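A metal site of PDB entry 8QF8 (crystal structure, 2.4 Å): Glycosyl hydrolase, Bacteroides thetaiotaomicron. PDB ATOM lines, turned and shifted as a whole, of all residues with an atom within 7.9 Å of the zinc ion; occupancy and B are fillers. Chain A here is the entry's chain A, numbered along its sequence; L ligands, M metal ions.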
ATOM      1  N   TRP A  79      -5.549  18.331  23.862  1.00  0.00           N
ATOM      2  CA  TRP A  79      -6.826  18.521  23.184  1.00  0.00           C
ATOM      3  C   TRP A  79      -6.752  18.106  21.712  1.00  0.00           C
ATOM      4  O   TRP A  79      -7.793  17.956  21.076  1.00  0.00           O
ATOM      5  CB  TRP A  79      -7.285  19.982  23.279  1.00  0.00           C
ATOM      6  CG  TRP A  79      -7.527  20.495  24.669  1.00  0.00           C
ATOM      7  CD1 TRP A  79      -7.238  19.921  25.879  1.00  0.00           C
ATOM      8  CD2 TRP A  79      -8.150  21.765  24.974  1.00  0.00           C
ATOM      9  NE1 TRP A  79      -7.627  20.749  26.900  1.00  0.00           N
ATOM     10  CE2 TRP A  79      -8.182  21.891  26.377  1.00  0.00           C
ATOM     11  CE3 TRP A  79      -8.682  22.800  24.193  1.00  0.00           C
ATOM     12  CZ2 TRP A  79      -8.716  23.008  27.013  1.00  0.00           C
ATOM     13  CZ3 TRP A  79      -9.235  23.897  24.816  1.00  0.00           C
ATOM     14  CH2 TRP A  79      -9.224  24.008  26.217  1.00  0.00           C
ATOM     15  N   HIS A  91      -5.131  28.018  14.230  1.00  0.00           N
ATOM     16  CA  HIS A  91      -4.443  29.153  14.838  1.00  0.00           C
ATOM     17  C   HIS A  91      -3.026  29.287  14.307  1.00  0.00           C
ATOM     18  O   HIS A  91      -2.556  30.408  14.111  1.00  0.00           O
ATOM     19  CB  HIS A  91      -4.371  29.001  16.364  1.00  0.00           C
ATOM     20  CG  HIS A  91      -5.649  29.221  17.109  1.00  0.00           C
ATOM     21  ND1 HIS A  91      -6.134  30.480  17.368  1.00  0.00           N
ATOM     22  CD2 HIS A  91      -6.483  28.359  17.717  1.00  0.00           C
ATOM     23  CE1 HIS A  91      -7.258  30.377  18.061  1.00  0.00           C
ATOM     24  NE2 HIS A  91      -7.487  29.099  18.285  1.00  0.00           N
ATOM     25  N   TYR A 164     -16.545  25.524  16.138  1.00  0.00           N
ATOM     26  CA  TYR A 164     -15.448  26.305  16.701  1.00  0.00           C
ATOM     27  C   TYR A 164     -14.122  25.878  16.069  1.00  0.00           C
ATOM     28  O   TYR A 164     -13.288  26.718  15.774  1.00  0.00           O
ATOM     29  CB  TYR A 164     -15.423  26.196  18.239  1.00  0.00           C
ATOM     30  CG  TYR A 164     -14.192  26.745  18.961  1.00  0.00           C
ATOM     31  CD1 TYR A 164     -12.998  26.032  19.005  1.00  0.00           C
ATOM     32  CD2 TYR A 164     -14.238  27.974  19.608  1.00  0.00           C
ATOM     33  CE1 TYR A 164     -11.874  26.555  19.629  1.00  0.00           C
ATOM     34  CE2 TYR A 164     -13.128  28.495  20.267  1.00  0.00           C
ATOM     35  CZ  TYR A 164     -11.941  27.783  20.270  1.00  0.00           C
ATOM     36  OH  TYR A 164     -10.842  28.288  20.905  1.00  0.00           O
ATOM     37  N   HIS A 262     -21.034  31.014  29.003  1.00  0.00           N
ATOM     38  CA  HIS A 262     -19.629  30.832  28.707  1.00  0.00           C
ATOM     39  C   HIS A 262     -19.201  32.014  27.846  1.00  0.00           C
ATOM     40  O   HIS A 262     -19.789  32.240  26.792  1.00  0.00           O
ATOM     41  CB  HIS A 262     -19.422  29.456  28.056  1.00  0.00           C
ATOM     42  CG  HIS A 262     -17.994  29.150  27.763  1.00  0.00           C
ATOM     43  ND1 HIS A 262     -17.394  29.621  26.613  1.00  0.00           N
ATOM     44  CD2 HIS A 262     -17.053  28.461  28.415  1.00  0.00           C
ATOM     45  CE1 HIS A 262     -16.133  29.218  26.599  1.00  0.00           C
ATOM     46  NE2 HIS A 262     -15.906  28.507  27.679  1.00  0.00           N
ATOM     47  N   ASN A 264     -16.177  33.250  26.315  1.00  0.00           N
ATOM     48  CA  ASN A 264     -15.426  33.200  25.071  1.00  0.00           C
ATOM     49  C   ASN A 264     -16.267  32.632  23.921  1.00  0.00           C
ATOM     50  O   ASN A 264     -15.922  32.851  22.763  1.00  0.00           O
ATOM     51  CB  ASN A 264     -14.127  32.399  25.204  1.00  0.00           C
ATOM     52  CG  ASN A 264     -13.132  32.746  24.108  1.00  0.00           C
ATOM     53  OD1 ASN A 264     -12.804  33.918  23.927  1.00  0.00           O
ATOM     54  ND2 ASN A 264     -12.713  31.765  23.324  1.00  0.00           N
ATOM     55  N   GLU A 318     -14.303  30.520  33.109  1.00  0.00           N
ATOM     56  CA  GLU A 318     -14.692  30.727  31.716  1.00  0.00           C
ATOM     57  C   GLU A 318     -16.093  31.314  31.548  1.00  0.00           C
ATOM     58  O   GLU A 318     -16.552  31.434  30.413  1.00  0.00           O
ATOM     59  CB  GLU A 318     -14.599  29.416  30.907  1.00  0.00           C
ATOM     60  CG  GLU A 318     -13.310  28.618  31.097  1.00  0.00           C
ATOM     61  CD  GLU A 318     -13.200  27.430  30.169  1.00  0.00           C
ATOM     62  OE1 GLU A 318     -14.133  27.178  29.395  1.00  0.00           O
ATOM     63  OE2 GLU A 318     -12.178  26.765  30.224  1.00  0.00           O
ATOM     64  N   GLU A 337      -9.934  34.396  31.605  1.00  0.00           N
ATOM     65  CA  GLU A 337      -9.319  33.604  30.561  1.00  0.00           C
ATOM     66  C   GLU A 337      -8.702  34.531  29.511  1.00  0.00           C
ATOM     67  O   GLU A 337      -9.283  35.573  29.201  1.00  0.00           O
ATOM     68  CB  GLU A 337     -10.385  32.702  29.926  1.00  0.00           C
ATOM     69  CG  GLU A 337      -9.853  31.866  28.783  1.00  0.00           C
ATOM     70  CD  GLU A 337     -10.877  31.060  28.026  1.00  0.00           C
ATOM     71  OE1 GLU A 337     -10.550  30.616  26.891  1.00  0.00           O
ATOM     72  OE2 GLU A 337     -12.001  30.894  28.543  1.00  0.00           O
ATOM     73  N   THR A 338      -7.556  34.136  28.941  1.00  0.00           N
ATOM     74  CA  THR A 338      -6.817  34.976  28.020  1.00  0.00           C
ATOM     75  C   THR A 338      -7.540  35.137  26.671  1.00  0.00           C
ATOM     76  O   THR A 338      -7.536  36.242  26.123  1.00  0.00           O
ATOM     77  CB  THR A 338      -5.378  34.484  27.821  1.00  0.00           C
ATOM     78  OG1 THR A 338      -4.866  34.030  29.075  1.00  0.00           O
ATOM     79  CG2 THR A 338      -4.465  35.562  27.297  1.00  0.00           C
ATOM     80  N   CYS A 339      -8.172  34.066  26.152  1.00  0.00           N
ATOM     81  CA  CYS A 339      -8.888  34.159  24.890  1.00  0.00           C
ATOM     82  C   CYS A 339      -9.889  35.319  24.881  1.00  0.00           C
ATOM     83  O   CYS A 339     -10.050  36.009  23.864  1.00  0.00           O
ATOM     84  CB  CYS A 339      -9.664  32.878  24.550  1.00  0.00           C
ATOM     85  SG  CYS A 339      -8.685  31.499  23.993  1.00  0.00           S
ATOM     86  N   ASN A 340     -10.564  35.526  26.023  1.00  0.00           N
ATOM     87  CA  ASN A 340     -11.617  36.517  26.129  1.00  0.00           C
ATOM     88  C   ASN A 340     -11.058  37.907  25.848  1.00  0.00           C
ATOM     89  O   ASN A 340     -11.692  38.682  25.147  1.00  0.00           O
ATOM     90  CB  ASN A 340     -12.329  36.464  27.484  1.00  0.00           C
ATOM     91  CG  ASN A 340     -12.747  35.078  27.913  1.00  0.00           C
ATOM     92  OD1 ASN A 340     -12.250  34.073  27.413  1.00  0.00           O
ATOM     93  ND2 ASN A 340     -13.639  35.012  28.893  1.00  0.00           N
ATOM     94  N   TYR A 342      -8.062  38.673  24.257  1.00  0.00           N
ATOM     95  CA  TYR A 342      -7.712  38.604  22.837  1.00  0.00           C
ATOM     96  C   TYR A 342      -8.916  38.998  21.974  1.00  0.00           C
ATOM     97  O   TYR A 342      -8.768  39.866  21.125  1.00  0.00           O
ATOM     98  CB  TYR A 342      -7.195  37.204  22.500  1.00  0.00           C
ATOM     99  CG  TYR A 342      -7.343  36.731  21.054  1.00  0.00           C
ATOM    100  CD1 TYR A 342      -8.408  35.916  20.687  1.00  0.00           C
ATOM    101  CD2 TYR A 342      -6.403  37.045  20.078  1.00  0.00           C
ATOM    102  CE1 TYR A 342      -8.554  35.463  19.384  1.00  0.00           C
ATOM    103  CE2 TYR A 342      -6.527  36.583  18.778  1.00  0.00           C
ATOM    104  CZ  TYR A 342      -7.612  35.791  18.433  1.00  0.00           C
ATOM    105  OH  TYR A 342      -7.773  35.329  17.153  1.00  0.00           O
ATOM    106  N   ASN A 343     -10.079  38.390  22.230  1.00  0.00           N
ATOM    107  CA  ASN A 343     -11.273  38.653  21.456  1.00  0.00           C
ATOM    108  C   ASN A 343     -11.875  40.023  21.751  1.00  0.00           C
ATOM    109  O   ASN A 343     -12.326  40.692  20.819  1.00  0.00           O
ATOM    110  CB  ASN A 343     -12.318  37.548  21.632  1.00  0.00           C
ATOM    111  CG  ASN A 343     -11.951  36.303  20.862  1.00  0.00           C
ATOM    112  OD1 ASN A 343     -11.629  36.391  19.673  1.00  0.00           O
ATOM    113  ND2 ASN A 343     -11.988  35.141  21.509  1.00  0.00           N
ATOM    114  N   VAL A 392      -0.427  31.654  29.237  1.00  0.00           N
ATOM    115  CA  VAL A 392      -1.340  31.510  30.359  1.00  0.00           C
ATOM    116  C   VAL A 392      -2.757  31.320  29.832  1.00  0.00           C
ATOM    117  O   VAL A 392      -3.166  31.945  28.856  1.00  0.00           O
ATOM    118  CB  VAL A 392      -1.246  32.749  31.274  1.00  0.00           C
ATOM    119  CG1 VAL A 392      -2.274  32.718  32.390  1.00  0.00           C
ATOM    120  CG2 VAL A 392       0.150  32.923  31.843  1.00  0.00           C
ATOM    121  N   TYR A 393      -3.524  30.470  30.534  1.00  0.00           N
ATOM    122  CA  TYR A 393      -4.947  30.266  30.292  1.00  0.00           C
ATOM    123  C   TYR A 393      -5.736  31.105  31.283  1.00  0.00           C
ATOM    124  O   TYR A 393      -6.525  31.957  30.885  1.00  0.00           O
ATOM    125  CB  TYR A 393      -5.215  28.758  30.355  1.00  0.00           C
ATOM    126  CG  TYR A 393      -6.551  28.230  29.865  1.00  0.00           C
ATOM    127  CD1 TYR A 393      -7.762  28.689  30.373  1.00  0.00           C
ATOM    128  CD2 TYR A 393      -6.609  27.206  28.916  1.00  0.00           C
ATOM    129  CE1 TYR A 393      -8.979  28.181  29.935  1.00  0.00           C
ATOM    130  CE2 TYR A 393      -7.825  26.690  28.476  1.00  0.00           C
ATOM    131  CZ  TYR A 393      -9.009  27.172  28.983  1.00  0.00           C
ATOM    132  OH  TYR A 393     -10.179  26.622  28.533  1.00  0.00           O
ATOM    133  N   PHE A 394      -5.511  30.861  32.589  1.00  0.00           N
ATOM    134  CA  PHE A 394      -6.225  31.539  33.656  1.00  0.00           C
ATOM    135  C   PHE A 394      -5.256  32.438  34.430  1.00  0.00           C
ATOM    136  O   PHE A 394      -4.172  31.995  34.819  1.00  0.00           O
ATOM    137  CB  PHE A 394      -6.854  30.524  34.610  1.00  0.00           C
ATOM    138  CG  PHE A 394      -8.057  29.757  34.097  1.00  0.00           C
ATOM    139  CD1 PHE A 394      -9.128  30.423  33.501  1.00  0.00           C
ATOM    140  CD2 PHE A 394      -8.144  28.379  34.260  1.00  0.00           C
ATOM    141  CE1 PHE A 394     -10.243  29.723  33.082  1.00  0.00           C
ATOM    142  CE2 PHE A 394      -9.262  27.681  33.831  1.00  0.00           C
ATOM    143  CZ  PHE A 394     -10.311  28.348  33.241  1.00  0.00           C
ATOM    144  N   TRP A 413      -4.260  24.082  24.237  1.00  0.00           N
ATOM    145  CA  TRP A 413      -5.436  24.753  24.752  1.00  0.00           C
ATOM    146  C   TRP A 413      -5.891  25.845  23.778  1.00  0.00           C
ATOM    147  O   TRP A 413      -5.101  26.308  22.974  1.00  0.00           O
ATOM    148  CB  TRP A 413      -5.185  25.423  26.112  1.00  0.00           C
ATOM    149  CG  TRP A 413      -4.362  24.622  27.080  1.00  0.00           C
ATOM    150  CD1 TRP A 413      -4.383  23.271  27.287  1.00  0.00           C
ATOM    151  CD2 TRP A 413      -3.394  25.164  27.990  1.00  0.00           C
ATOM    152  NE1 TRP A 413      -3.483  22.944  28.251  1.00  0.00           N
ATOM    153  CE2 TRP A 413      -2.865  24.076  28.704  1.00  0.00           C
ATOM    154  CE3 TRP A 413      -2.922  26.450  28.254  1.00  0.00           C
ATOM    155  CZ2 TRP A 413      -1.878  24.233  29.674  1.00  0.00           C
ATOM    156  CZ3 TRP A 413      -1.958  26.616  29.221  1.00  0.00           C
ATOM    157  CH2 TRP A 413      -1.439  25.519  29.925  1.00  0.00           C
ATOM    158  N   CYS A 414      -7.120  26.329  23.988  1.00  0.00           N
ATOM    159  CA  CYS A 414      -7.639  27.480  23.278  1.00  0.00           C
ATOM    160  C   CYS A 414      -6.737  28.696  23.506  1.00  0.00           C
ATOM    161  O   CYS A 414      -6.470  29.456  22.579  1.00  0.00           O
ATOM    162  CB  CYS A 414      -9.083  27.805  23.676  1.00  0.00           C
ATOM    163  SG  CYS A 414      -9.538  27.851  25.402  1.00  0.00           S
ATOM    164  N   CYS A 415      -6.277  28.866  24.764  1.00  0.00           N
ATOM    165  CA  CYS A 415      -5.439  30.001  25.124  1.00  0.00           C
ATOM    166  C   CYS A 415      -4.009  29.879  24.572  1.00  0.00           C
ATOM    167  O   CYS A 415      -3.294  30.890  24.533  1.00  0.00           O
ATOM    168  CB  CYS A 415      -5.455  30.200  26.639  1.00  0.00           C
ATOM    169  SG  CYS A 415      -7.020  30.780  27.253  1.00  0.00           S
ATOM    170  N   VAL A 416      -3.575  28.674  24.149  1.00  0.00           N
ATOM    171  CA  VAL A 416      -2.352  28.543  23.367  1.00  0.00           C
ATOM    172  C   VAL A 416      -2.581  29.102  21.958  1.00  0.00           C
ATOM    173  O   VAL A 416      -1.809  29.927  21.482  1.00  0.00           O
ATOM    174  CB  VAL A 416      -1.845  27.096  23.318  1.00  0.00           C
ATOM    175  CG1 VAL A 416      -0.658  26.939  22.367  1.00  0.00           C
ATOM    176  CG2 VAL A 416      -1.483  26.581  24.707  1.00  0.00           C
ATOM    177  N   GLY A 417      -3.672  28.663  21.318  1.00  0.00           N
ATOM    178  CA  GLY A 417      -4.057  29.143  19.999  1.00  0.00           C
ATOM    179  C   GLY A 417      -4.094  30.672  19.875  1.00  0.00           C
ATOM    180  O   GLY A 417      -3.403  31.247  19.041  1.00  0.00           O
ATOM    181  N   SER A 418      -4.883  31.321  20.729  1.00  0.00           N
ATOM    182  CA  SER A 418      -4.926  32.775  20.778  1.00  0.00           C
ATOM    183  C   SER A 418      -3.595  33.363  21.243  1.00  0.00           C
ATOM    184  O   SER A 418      -3.224  34.457  20.818  1.00  0.00           O
ATOM    185  CB  SER A 418      -6.063  33.249  21.644  1.00  0.00           C
ATOM    186  OG  SER A 418      -5.958  32.680  22.931  1.00  0.00           O
ATOM    187  N   GLY A 419      -2.892  32.634  22.132  1.00  0.00           N
ATOM    188  CA  GLY A 419      -1.576  33.028  22.600  1.00  0.00           C
ATOM    189  C   GLY A 419      -0.565  33.181  21.457  1.00  0.00           C
ATOM    190  O   GLY A 419       0.204  34.141  21.434  1.00  0.00           O
ATOM    191  N   HIS A 580      -4.033  23.173  32.443  1.00  0.00           N
ATOM    192  CA  HIS A 580      -4.107  24.631  32.330  1.00  0.00           C
ATOM    193  C   HIS A 580      -4.415  25.334  33.659  1.00  0.00           C
ATOM    194  O   HIS A 580      -4.176  26.537  33.753  1.00  0.00           O
ATOM    195  CB  HIS A 580      -5.115  25.041  31.255  1.00  0.00           C
ATOM    196  CG  HIS A 580      -6.530  24.676  31.509  1.00  0.00           C
ATOM    197  ND1 HIS A 580      -6.982  23.372  31.448  1.00  0.00           N
ATOM    198  CD2 HIS A 580      -7.592  25.444  31.790  1.00  0.00           C
ATOM    199  CE1 HIS A 580      -8.279  23.370  31.700  1.00  0.00           C
ATOM    200  NE2 HIS A 580      -8.679  24.616  31.903  1.00  0.00           N
HETATM  201  C1  LIG L   1     -13.789  25.988  22.849  1.00  0.00           C
HETATM  202  C2  LIG L   1     -12.815  26.916  23.566  1.00  0.00           C
HETATM  203  C3  LIG L   1     -11.829  26.249  24.544  1.00  0.00           C
HETATM  204  C4  LIG L   1     -11.335  27.359  25.531  1.00  0.00           C
HETATM  205  C5  LIG L   1     -12.376  28.494  25.344  1.00  0.00           C
HETATM  206  O1  LIG L   1     -14.685  25.372  23.763  1.00  0.00           O
HETATM  207  C6  LIG L   1     -13.492  28.005  24.408  1.00  0.00           C
HETATM  208  O2  LIG L   1     -13.933  29.120  23.639  1.00  0.00           O
HETATM  209  N1  LIG L   1     -12.409  25.071  25.260  1.00  0.00           N
HETATM  210  O3  LIG L   1     -13.014  28.951  26.545  1.00  0.00           O
HETATM  211 ZN    ZN M   1      -8.803  30.205  25.972  1.00  0.00          ZN
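The side-chain carboxylate (OE2) of Glu 337 is in hydrogen-bond range of an oxygen (O3) of the ligand. SG of Cys 414 is covalently linked to C4 of the ligand (1.9 Å). ND2 of Asn 264 is in hydrogen-bond range of O2 of the ligand (2.9 Å). O3 of the ligand lies close to NE2 of His 262 (3.1 Å).
The side-chain amide oxygen (OD1) of Asn 340 sits close to the side-chain carboxylate (OE2) of Glu 337. The side-chain sulfur of Cys 415 sits close to the backbone NH of Thr 338, at 3.8 Å. The side-chain hydroxyl (OG) of Ser 418 sits close to the side-chain sulfur (SG) of Cys 339, 3.2 Å away. OD1 of Asn 264 lies close to O of Cys 339, 3.5 Å away. O of Cys 339 lies within hydrogen-bond range of ND2 of Asn 343. SG of Cys 414 sits close to OH of Tyr 393 (3.4 Å). The backbone carbonyl oxygen (O) of Cys 414 sits at hydrogen-bond distance from the side-chain hydroxyl (OG) of Ser 418 (3.3 Å).
Of the 23 residues printed, 4 come within 4 Å of the zinc ion. Along chain A the residues within 4 Å of the zinc ion span positions 337 to 415.
The zinc ion is bound by OE1 of Glu 337 (2.0 Å), SG of Cys 415 (2.3 Å), SG of Cys 339 (2.4 Å) and SG of Cys 414 (2.5 Å).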
